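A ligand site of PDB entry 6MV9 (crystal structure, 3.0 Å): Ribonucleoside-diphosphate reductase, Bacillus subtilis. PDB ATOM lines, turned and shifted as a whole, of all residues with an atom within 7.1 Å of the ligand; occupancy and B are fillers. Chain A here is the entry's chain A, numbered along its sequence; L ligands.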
ATOM      1  N   ASP A  29     -27.439  23.528  21.753  1.00  0.00           N
ATOM      2  CA  ASP A  29     -26.599  24.648  21.353  1.00  0.00           C
ATOM      3  C   ASP A  29     -25.170  24.191  21.084  1.00  0.00           C
ATOM      4  O   ASP A  29     -24.460  24.807  20.276  1.00  0.00           O
ATOM      5  CB  ASP A  29     -26.613  25.731  22.434  1.00  0.00           C
ATOM      6  CG  ASP A  29     -26.687  27.135  21.872  1.00  0.00           C
ATOM      7  OD1 ASP A  29     -26.960  27.272  20.659  1.00  0.00           O
ATOM      8  OD2 ASP A  29     -26.480  28.097  22.638  1.00  0.00           O
ATOM      9  N   LYS A  30     -24.737  23.113  21.750  1.00  0.00           N
ATOM     10  CA  LYS A  30     -23.410  22.556  21.521  1.00  0.00           C
ATOM     11  C   LYS A  30     -23.254  22.075  20.084  1.00  0.00           C
ATOM     12  O   LYS A  30     -22.172  22.188  19.499  1.00  0.00           O
ATOM     13  CB  LYS A  30     -23.179  21.421  22.527  1.00  0.00           C
ATOM     14  CG  LYS A  30     -21.918  20.588  22.352  1.00  0.00           C
ATOM     15  CD  LYS A  30     -22.235  19.272  21.640  1.00  0.00           C
ATOM     16  CE  LYS A  30     -21.080  18.289  21.726  1.00  0.00           C
ATOM     17  NZ  LYS A  30     -21.444  16.967  21.128  1.00  0.00           N
ATOM     18  N   VAL A  33     -23.303  25.372  17.428  1.00  0.00           N
ATOM     19  CA  VAL A  33     -22.037  26.073  17.268  1.00  0.00           C
ATOM     20  C   VAL A  33     -21.070  25.245  16.455  1.00  0.00           C
ATOM     21  O   VAL A  33     -20.210  25.789  15.755  1.00  0.00           O
ATOM     22  CB  VAL A  33     -21.462  26.451  18.653  1.00  0.00           C
ATOM     23  CG1 VAL A  33     -21.015  25.208  19.413  1.00  0.00           C
ATOM     24  CG2 VAL A  33     -20.302  27.437  18.504  1.00  0.00           C
ATOM     25  N   HIS A  34     -21.174  23.917  16.516  1.00  0.00           N
ATOM     26  CA  HIS A  34     -20.349  23.072  15.662  1.00  0.00           C
ATOM     27  C   HIS A  34     -20.761  23.226  14.203  1.00  0.00           C
ATOM     28  O   HIS A  34     -19.895  23.326  13.320  1.00  0.00           O
ATOM     29  CB  HIS A  34     -20.452  21.611  16.105  1.00  0.00           C
ATOM     30  CG  HIS A  34     -19.452  20.716  15.458  1.00  0.00           C
ATOM     31  ND1 HIS A  34     -19.661  20.101  14.241  1.00  0.00           N
ATOM     32  CD2 HIS A  34     -18.221  20.316  15.868  1.00  0.00           C
ATOM     33  CE1 HIS A  34     -18.616  19.377  13.927  1.00  0.00           C
ATOM     34  NE2 HIS A  34     -17.724  19.476  14.898  1.00  0.00           N
ATOM     35  N   SER A  35     -22.060  23.252  13.935  1.00  0.00           N
ATOM     36  CA  SER A  35     -22.583  23.482  12.583  1.00  0.00           C
ATOM     37  C   SER A  35     -22.358  24.900  12.089  1.00  0.00           C
ATOM     38  O   SER A  35     -22.694  25.182  10.933  1.00  0.00           O
ATOM     39  CB  SER A  35     -24.086  23.163  12.543  1.00  0.00           C
ATOM     40  OG  SER A  35     -24.647  23.509  11.289  1.00  0.00           O
ATOM     41  N   TYR A  36     -21.815  25.788  12.924  1.00  0.00           N
ATOM     42  CA  TYR A  36     -21.467  27.132  12.496  1.00  0.00           C
ATOM     43  C   TYR A  36     -20.006  27.226  12.072  1.00  0.00           C
ATOM     44  O   TYR A  36     -19.683  27.934  11.112  1.00  0.00           O
ATOM     45  CB  TYR A  36     -21.761  28.131  13.613  1.00  0.00           C
ATOM     46  CG  TYR A  36     -21.548  29.589  13.236  1.00  0.00           C
ATOM     47  CD1 TYR A  36     -22.371  30.217  12.315  1.00  0.00           C
ATOM     48  CD2 TYR A  36     -20.539  30.333  13.829  1.00  0.00           C
ATOM     49  CE1 TYR A  36     -22.179  31.546  11.973  1.00  0.00           C
ATOM     50  CE2 TYR A  36     -20.347  31.665  13.510  1.00  0.00           C
ATOM     51  CZ  TYR A  36     -21.162  32.272  12.579  1.00  0.00           C
ATOM     52  OH  TYR A  36     -20.974  33.593  12.253  1.00  0.00           O
ATOM     53  N   PHE A  37     -19.113  26.503  12.759  1.00  0.00           N
ATOM     54  CA  PHE A  37     -17.713  26.490  12.365  1.00  0.00           C
ATOM     55  C   PHE A  37     -17.513  25.694  11.082  1.00  0.00           C
ATOM     56  O   PHE A  37     -16.814  26.135  10.171  1.00  0.00           O
ATOM     57  CB  PHE A  37     -16.850  25.937  13.492  1.00  0.00           C
ATOM     58  CG  PHE A  37     -16.593  26.927  14.591  1.00  0.00           C
ATOM     59  CD1 PHE A  37     -15.355  27.552  14.708  1.00  0.00           C
ATOM     60  CD2 PHE A  37     -17.588  27.247  15.510  1.00  0.00           C
ATOM     61  CE1 PHE A  37     -15.121  28.469  15.710  1.00  0.00           C
ATOM     62  CE2 PHE A  37     -17.354  28.164  16.511  1.00  0.00           C
ATOM     63  CZ  PHE A  37     -16.120  28.777  16.622  1.00  0.00           C
ATOM     64  N   VAL A  38     -18.134  24.523  10.992  1.00  0.00           N
ATOM     65  CA  VAL A  38     -18.225  23.821   9.715  1.00  0.00           C
ATOM     66  C   VAL A  38     -19.390  24.426   8.923  1.00  0.00           C
ATOM     67  O   VAL A  38     -20.330  24.967   9.498  1.00  0.00           O
ATOM     68  CB  VAL A  38     -18.414  22.307   9.938  1.00  0.00           C
ATOM     69  CG1 VAL A  38     -18.094  21.539   8.660  1.00  0.00           C
ATOM     70  CG2 VAL A  38     -17.548  21.831  11.091  1.00  0.00           C
ATOM     71  N   ILE A  41     -17.790  29.360   8.703  1.00  0.00           N
ATOM     72  CA  ILE A  41     -16.649  30.228   8.980  1.00  0.00           C
ATOM     73  C   ILE A  41     -15.339  29.549   8.603  1.00  0.00           C
ATOM     74  O   ILE A  41     -14.367  30.228   8.267  1.00  0.00           O
ATOM     75  CB  ILE A  41     -16.640  30.679  10.458  1.00  0.00           C
ATOM     76  CG1 ILE A  41     -16.024  29.619  11.367  1.00  0.00           C
ATOM     77  CG2 ILE A  41     -18.027  31.056  10.927  1.00  0.00           C
ATOM     78  CD1 ILE A  41     -15.424  30.201  12.610  1.00  0.00           C
ATOM     79  N   ASN A  42     -15.285  28.207   8.634  1.00  0.00           N
ATOM     80  CA  ASN A  42     -14.117  27.532   8.101  1.00  0.00           C
ATOM     81  C   ASN A  42     -14.057  27.638   6.587  1.00  0.00           C
ATOM     82  O   ASN A  42     -12.970  27.712   6.010  1.00  0.00           O
ATOM     83  CB  ASN A  42     -14.114  26.064   8.543  1.00  0.00           C
ATOM     84  CG  ASN A  42     -13.783  25.900  10.005  1.00  0.00           C
ATOM     85  OD1 ASN A  42     -13.034  26.685  10.577  1.00  0.00           O
ATOM     86  ND2 ASN A  42     -14.351  24.868  10.625  1.00  0.00           N
ATOM     87  N   TYR A  85      -3.390  28.810  21.020  1.00  0.00           N
ATOM     88  CA  TYR A  85      -4.026  27.571  20.575  1.00  0.00           C
ATOM     89  C   TYR A  85      -3.761  26.408  21.520  1.00  0.00           C
ATOM     90  O   TYR A  85      -4.479  25.413  21.453  1.00  0.00           O
ATOM     91  CB  TYR A  85      -3.553  27.220  19.163  1.00  0.00           C
ATOM     92  CG  TYR A  85      -4.022  28.190  18.106  1.00  0.00           C
ATOM     93  CD1 TYR A  85      -5.254  28.039  17.498  1.00  0.00           C
ATOM     94  CD2 TYR A  85      -3.221  29.266  17.717  1.00  0.00           C
ATOM     95  CE1 TYR A  85      -5.685  28.919  16.538  1.00  0.00           C
ATOM     96  CE2 TYR A  85      -3.645  30.156  16.750  1.00  0.00           C
ATOM     97  CZ  TYR A  85      -4.876  29.978  16.161  1.00  0.00           C
ATOM     98  OH  TYR A  85      -5.311  30.846  15.195  1.00  0.00           O
ATOM     99  N   LYS A  88      -7.319  24.267  23.817  1.00  0.00           N
ATOM    100  CA  LYS A  88      -8.266  24.059  22.694  1.00  0.00           C
ATOM    101  C   LYS A  88      -9.577  24.690  23.144  1.00  0.00           C
ATOM    102  O   LYS A  88     -10.419  23.998  23.753  1.00  0.00           O
ATOM    103  CB  LYS A  88      -8.434  22.574  22.393  1.00  0.00           C
ATOM    104  N   PHE A  89      -9.714  25.990  22.840  1.00  0.00           N
ATOM    105  CA  PHE A  89     -10.855  26.777  23.289  1.00  0.00           C
ATOM    106  C   PHE A  89     -12.035  26.553  22.359  1.00  0.00           C
ATOM    107  O   PHE A  89     -11.881  26.623  21.133  1.00  0.00           O
ATOM    108  CB  PHE A  89     -10.497  28.264  23.344  1.00  0.00           C
ATOM    109  CG  PHE A  89     -11.663  29.153  23.697  1.00  0.00           C
ATOM    110  CD1 PHE A  89     -12.444  29.723  22.707  1.00  0.00           C
ATOM    111  CD2 PHE A  89     -11.991  29.394  25.015  1.00  0.00           C
ATOM    112  CE1 PHE A  89     -13.517  30.524  23.017  1.00  0.00           C
ATOM    113  CE2 PHE A  89     -13.063  30.200  25.347  1.00  0.00           C
ATOM    114  CZ  PHE A  89     -13.827  30.770  24.346  1.00  0.00           C
ATOM    115  N   ARG A  90     -13.214  26.301  22.932  1.00  0.00           N
ATOM    116  CA  ARG A  90     -14.411  26.087  22.128  1.00  0.00           C
ATOM    117  C   ARG A  90     -15.556  26.925  22.687  1.00  0.00           C
ATOM    118  O   ARG A  90     -15.820  26.917  23.889  1.00  0.00           O
ATOM    119  CB  ARG A  90     -14.813  24.609  22.098  1.00  0.00           C
ATOM    120  CG  ARG A  90     -13.619  23.678  21.942  1.00  0.00           C
ATOM    121  CD  ARG A  90     -13.307  23.370  20.497  1.00  0.00           C
ATOM    122  NE  ARG A  90     -11.981  23.906  20.178  1.00  0.00           N
ATOM    123  CZ  ARG A  90     -11.225  23.506  19.172  1.00  0.00           C
ATOM    124  NH1 ARG A  90     -11.650  22.556  18.355  1.00  0.00           N
ATOM    125  NH2 ARG A  90     -10.034  24.056  18.979  1.00  0.00           N
ATOM    126  N   PHE A  91     -16.234  27.651  21.796  1.00  0.00           N
ATOM    127  CA  PHE A  91     -17.406  28.417  22.211  1.00  0.00           C
ATOM    128  C   PHE A  91     -18.523  27.466  22.624  1.00  0.00           C
ATOM    129  O   PHE A  91     -18.898  26.582  21.854  1.00  0.00           O
ATOM    130  CB  PHE A  91     -17.892  29.306  21.065  1.00  0.00           C
ATOM    131  CG  PHE A  91     -17.066  30.543  20.858  1.00  0.00           C
ATOM    132  CD1 PHE A  91     -17.262  31.668  21.643  1.00  0.00           C
ATOM    133  CD2 PHE A  91     -16.091  30.586  19.865  1.00  0.00           C
ATOM    134  CE1 PHE A  91     -16.509  32.804  21.447  1.00  0.00           C
ATOM    135  CE2 PHE A  91     -15.338  31.722  19.669  1.00  0.00           C
ATOM    136  CZ  PHE A  91     -15.541  32.837  20.460  1.00  0.00           C
ATOM    137  N   PRO A  92     -19.084  27.632  23.826  1.00  0.00           N
ATOM    138  CA  PRO A  92     -20.152  26.703  24.264  1.00  0.00           C
ATOM    139  C   PRO A  92     -21.504  26.975  23.650  1.00  0.00           C
ATOM    140  O   PRO A  92     -22.350  26.063  23.626  1.00  0.00           O
ATOM    141  CB  PRO A  92     -20.183  26.919  25.781  1.00  0.00           C
ATOM    142  CG  PRO A  92     -19.760  28.335  25.959  1.00  0.00           C
ATOM    143  CD  PRO A  92     -18.741  28.614  24.876  1.00  0.00           C
ATOM    144  N   SER A  93     -21.756  28.182  23.153  1.00  0.00           N
ATOM    145  CA  SER A  93     -23.038  28.544  22.580  1.00  0.00           C
ATOM    146  C   SER A  93     -22.841  29.091  21.177  1.00  0.00           C
ATOM    147  O   SER A  93     -21.727  29.461  20.790  1.00  0.00           O
ATOM    148  CB  SER A  93     -23.783  29.569  23.458  1.00  0.00           C
ATOM    149  OG  SER A  93     -22.942  30.655  23.810  1.00  0.00           O
ATOM    150  N   ALA A  97     -19.979  32.677  19.663  1.00  0.00           N
ATOM    151  CA  ALA A  97     -19.102  32.811  18.512  1.00  0.00           C
ATOM    152  C   ALA A  97     -19.676  33.769  17.473  1.00  0.00           C
ATOM    153  O   ALA A  97     -18.918  34.431  16.767  1.00  0.00           O
ATOM    154  CB  ALA A  97     -18.845  31.445  17.876  1.00  0.00           C
ATOM    155  N   TYR A 101     -17.284  36.756  15.625  1.00  0.00           N
ATOM    156  CA  TYR A 101     -16.951  36.775  14.210  1.00  0.00           C
ATOM    157  C   TYR A 101     -17.760  37.795  13.403  1.00  0.00           C
ATOM    158  O   TYR A 101     -17.619  37.822  12.174  1.00  0.00           O
ATOM    159  CB  TYR A 101     -17.125  35.377  13.614  1.00  0.00           C
ATOM    160  CG  TYR A 101     -15.993  34.451  13.973  1.00  0.00           C
ATOM    161  CD1 TYR A 101     -16.129  33.525  15.000  1.00  0.00           C
ATOM    162  CD2 TYR A 101     -14.773  34.517  13.306  1.00  0.00           C
ATOM    163  CE1 TYR A 101     -15.087  32.684  15.330  1.00  0.00           C
ATOM    164  CE2 TYR A 101     -13.732  33.687  13.635  1.00  0.00           C
ATOM    165  CZ  TYR A 101     -13.888  32.765  14.648  1.00  0.00           C
ATOM    166  OH  TYR A 101     -12.851  31.936  14.990  1.00  0.00           O
ATOM    167  N   ARG A 117      -9.137  34.833  13.713  1.00  0.00           N
ATOM    168  CA  ARG A 117      -9.951  34.025  14.612  1.00  0.00           C
ATOM    169  C   ARG A 117      -9.640  34.416  16.044  1.00  0.00           C
ATOM    170  O   ARG A 117      -8.698  35.173  16.315  1.00  0.00           O
ATOM    171  CB  ARG A 117      -9.694  32.531  14.393  1.00  0.00           C
ATOM    172  CG  ARG A 117      -9.865  32.065  12.957  1.00  0.00           C
ATOM    173  CD  ARG A 117      -9.468  30.608  12.776  1.00  0.00           C
ATOM    174  NE  ARG A 117     -10.620  29.751  12.502  1.00  0.00           N
ATOM    175  CZ  ARG A 117     -11.185  28.933  13.386  1.00  0.00           C
ATOM    176  NH1 ARG A 117     -10.704  28.849  14.616  1.00  0.00           N
ATOM    177  NH2 ARG A 117     -12.231  28.199  13.039  1.00  0.00           N
ATOM    178  N   GLU A 119      -7.896  33.555  19.491  1.00  0.00           N
ATOM    179  CA  GLU A 119      -6.494  33.166  19.663  1.00  0.00           C
ATOM    180  C   GLU A 119      -5.580  34.049  18.816  1.00  0.00           C
ATOM    181  O   GLU A 119      -4.481  34.417  19.253  1.00  0.00           O
ATOM    182  CB  GLU A 119      -6.243  31.683  19.338  1.00  0.00           C
ATOM    183  CG  GLU A 119      -6.750  30.699  20.387  1.00  0.00           C
ATOM    184  CD  GLU A 119      -7.805  29.732  19.844  1.00  0.00           C
ATOM    185  OE1 GLU A 119      -8.293  29.945  18.703  1.00  0.00           O
ATOM    186  OE2 GLU A 119      -8.146  28.759  20.551  1.00  0.00           O
HETATM  187  P1  LIG L   1     -11.806  18.804  16.958  1.00  0.00           P
HETATM  188  O1  LIG L   1     -11.781  19.265  18.423  1.00  0.00           O
HETATM  189  O2  LIG L   1     -10.829  19.542  16.112  1.00  0.00           O
HETATM  190  O3  LIG L   1     -11.597  17.288  16.930  1.00  0.00           O
HETATM  191  P2  LIG L   1     -13.902  19.297  14.995  1.00  0.00           P
HETATM  192  O4  LIG L   1     -13.123  18.575  13.955  1.00  0.00           O
HETATM  193  O5  LIG L   1     -15.378  18.907  15.054  1.00  0.00           O
HETATM  194  O6  LIG L   1     -13.295  19.055  16.444  1.00  0.00           O
HETATM  195  O7  LIG L   1     -13.863  20.884  14.723  1.00  0.00           O
HETATM  196  C1  LIG L   1     -13.359  21.479  13.517  1.00  0.00           C
HETATM  197  C2  LIG L   1     -12.689  22.790  13.827  1.00  0.00           C
HETATM  198  O8  LIG L   1     -13.684  23.834  13.892  1.00  0.00           O
HETATM  199  C3  LIG L   1     -11.958  22.853  15.167  1.00  0.00           C
HETATM  200  O9  LIG L   1     -10.605  22.423  15.044  1.00  0.00           O
HETATM  201  C4  LIG L   1     -12.057  24.327  15.547  1.00  0.00           C
HETATM  202  O10 LIG L   1     -11.059  25.104  14.893  1.00  0.00           O
HETATM  203  C5  LIG L   1     -13.447  24.670  15.009  1.00  0.00           C
HETATM  204  N1  LIG L   1     -14.533  24.503  15.970  1.00  0.00           N
HETATM  205  C6  LIG L   1     -15.623  23.673  15.855  1.00  0.00           C
HETATM  206  N2  LIG L   1     -16.506  23.811  16.816  1.00  0.00           N
HETATM  207  C7  LIG L   1     -15.959  24.797  17.622  1.00  0.00           C
HETATM  208  C8  LIG L   1     -16.428  25.441  18.785  1.00  0.00           C
HETATM  209  N3  LIG L   1     -17.589  25.145  19.383  1.00  0.00           N
HETATM  210  N4  LIG L   1     -15.660  26.417  19.318  1.00  0.00           N
HETATM  211  C9  LIG L   1     -14.494  26.716  18.727  1.00  0.00           C
HETATM  212  N5  LIG L   1     -13.955  26.175  17.627  1.00  0.00           N
HETATM  213  C10 LIG L   1     -14.740  25.223  17.122  1.00  0.00           C
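Merely in contact with the ligand: Phe 37 (3.2 Å), Val 33 (3.4 Å), Phe 89 (3.6 Å) and Arg 117 (3.8 Å).
Hydrophobic or aromatic side chains within 4 Å of the ligand: Val 33, His 34 and Phe 37.
Eight residues have an atom within 4 Å of the ligand: Val 33, His 34, Phe 37, Asn 42, Phe 89, Arg 90, Phe 91 and Arg 117.
The side-chain amide oxygen of Asn 42 sits at hydrogen-bond distance from the guanidinium group of Arg 117.
O of Phe 37 sits at hydrogen-bond distance from ND2 of Asn 42 (2.8 Å).
O of Phe 91 sits at hydrogen-bond distance from N3 of the ligand.
The guanidinium group of Arg 90 lies within salt-bridge range of an oxygen (O1) of the ligand, at 3.3 Å.
O5 of the ligand is in hydrogen-bond range of NE2 of His 34.
ND2 of Asn 42 is in hydrogen-bond range of O8 of the ligand (3.5 Å).
The backbone NH (N) of Phe 91 sits at hydrogen-bond distance from a nitrogen (N4) of the ligand, at 2.8 Å.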
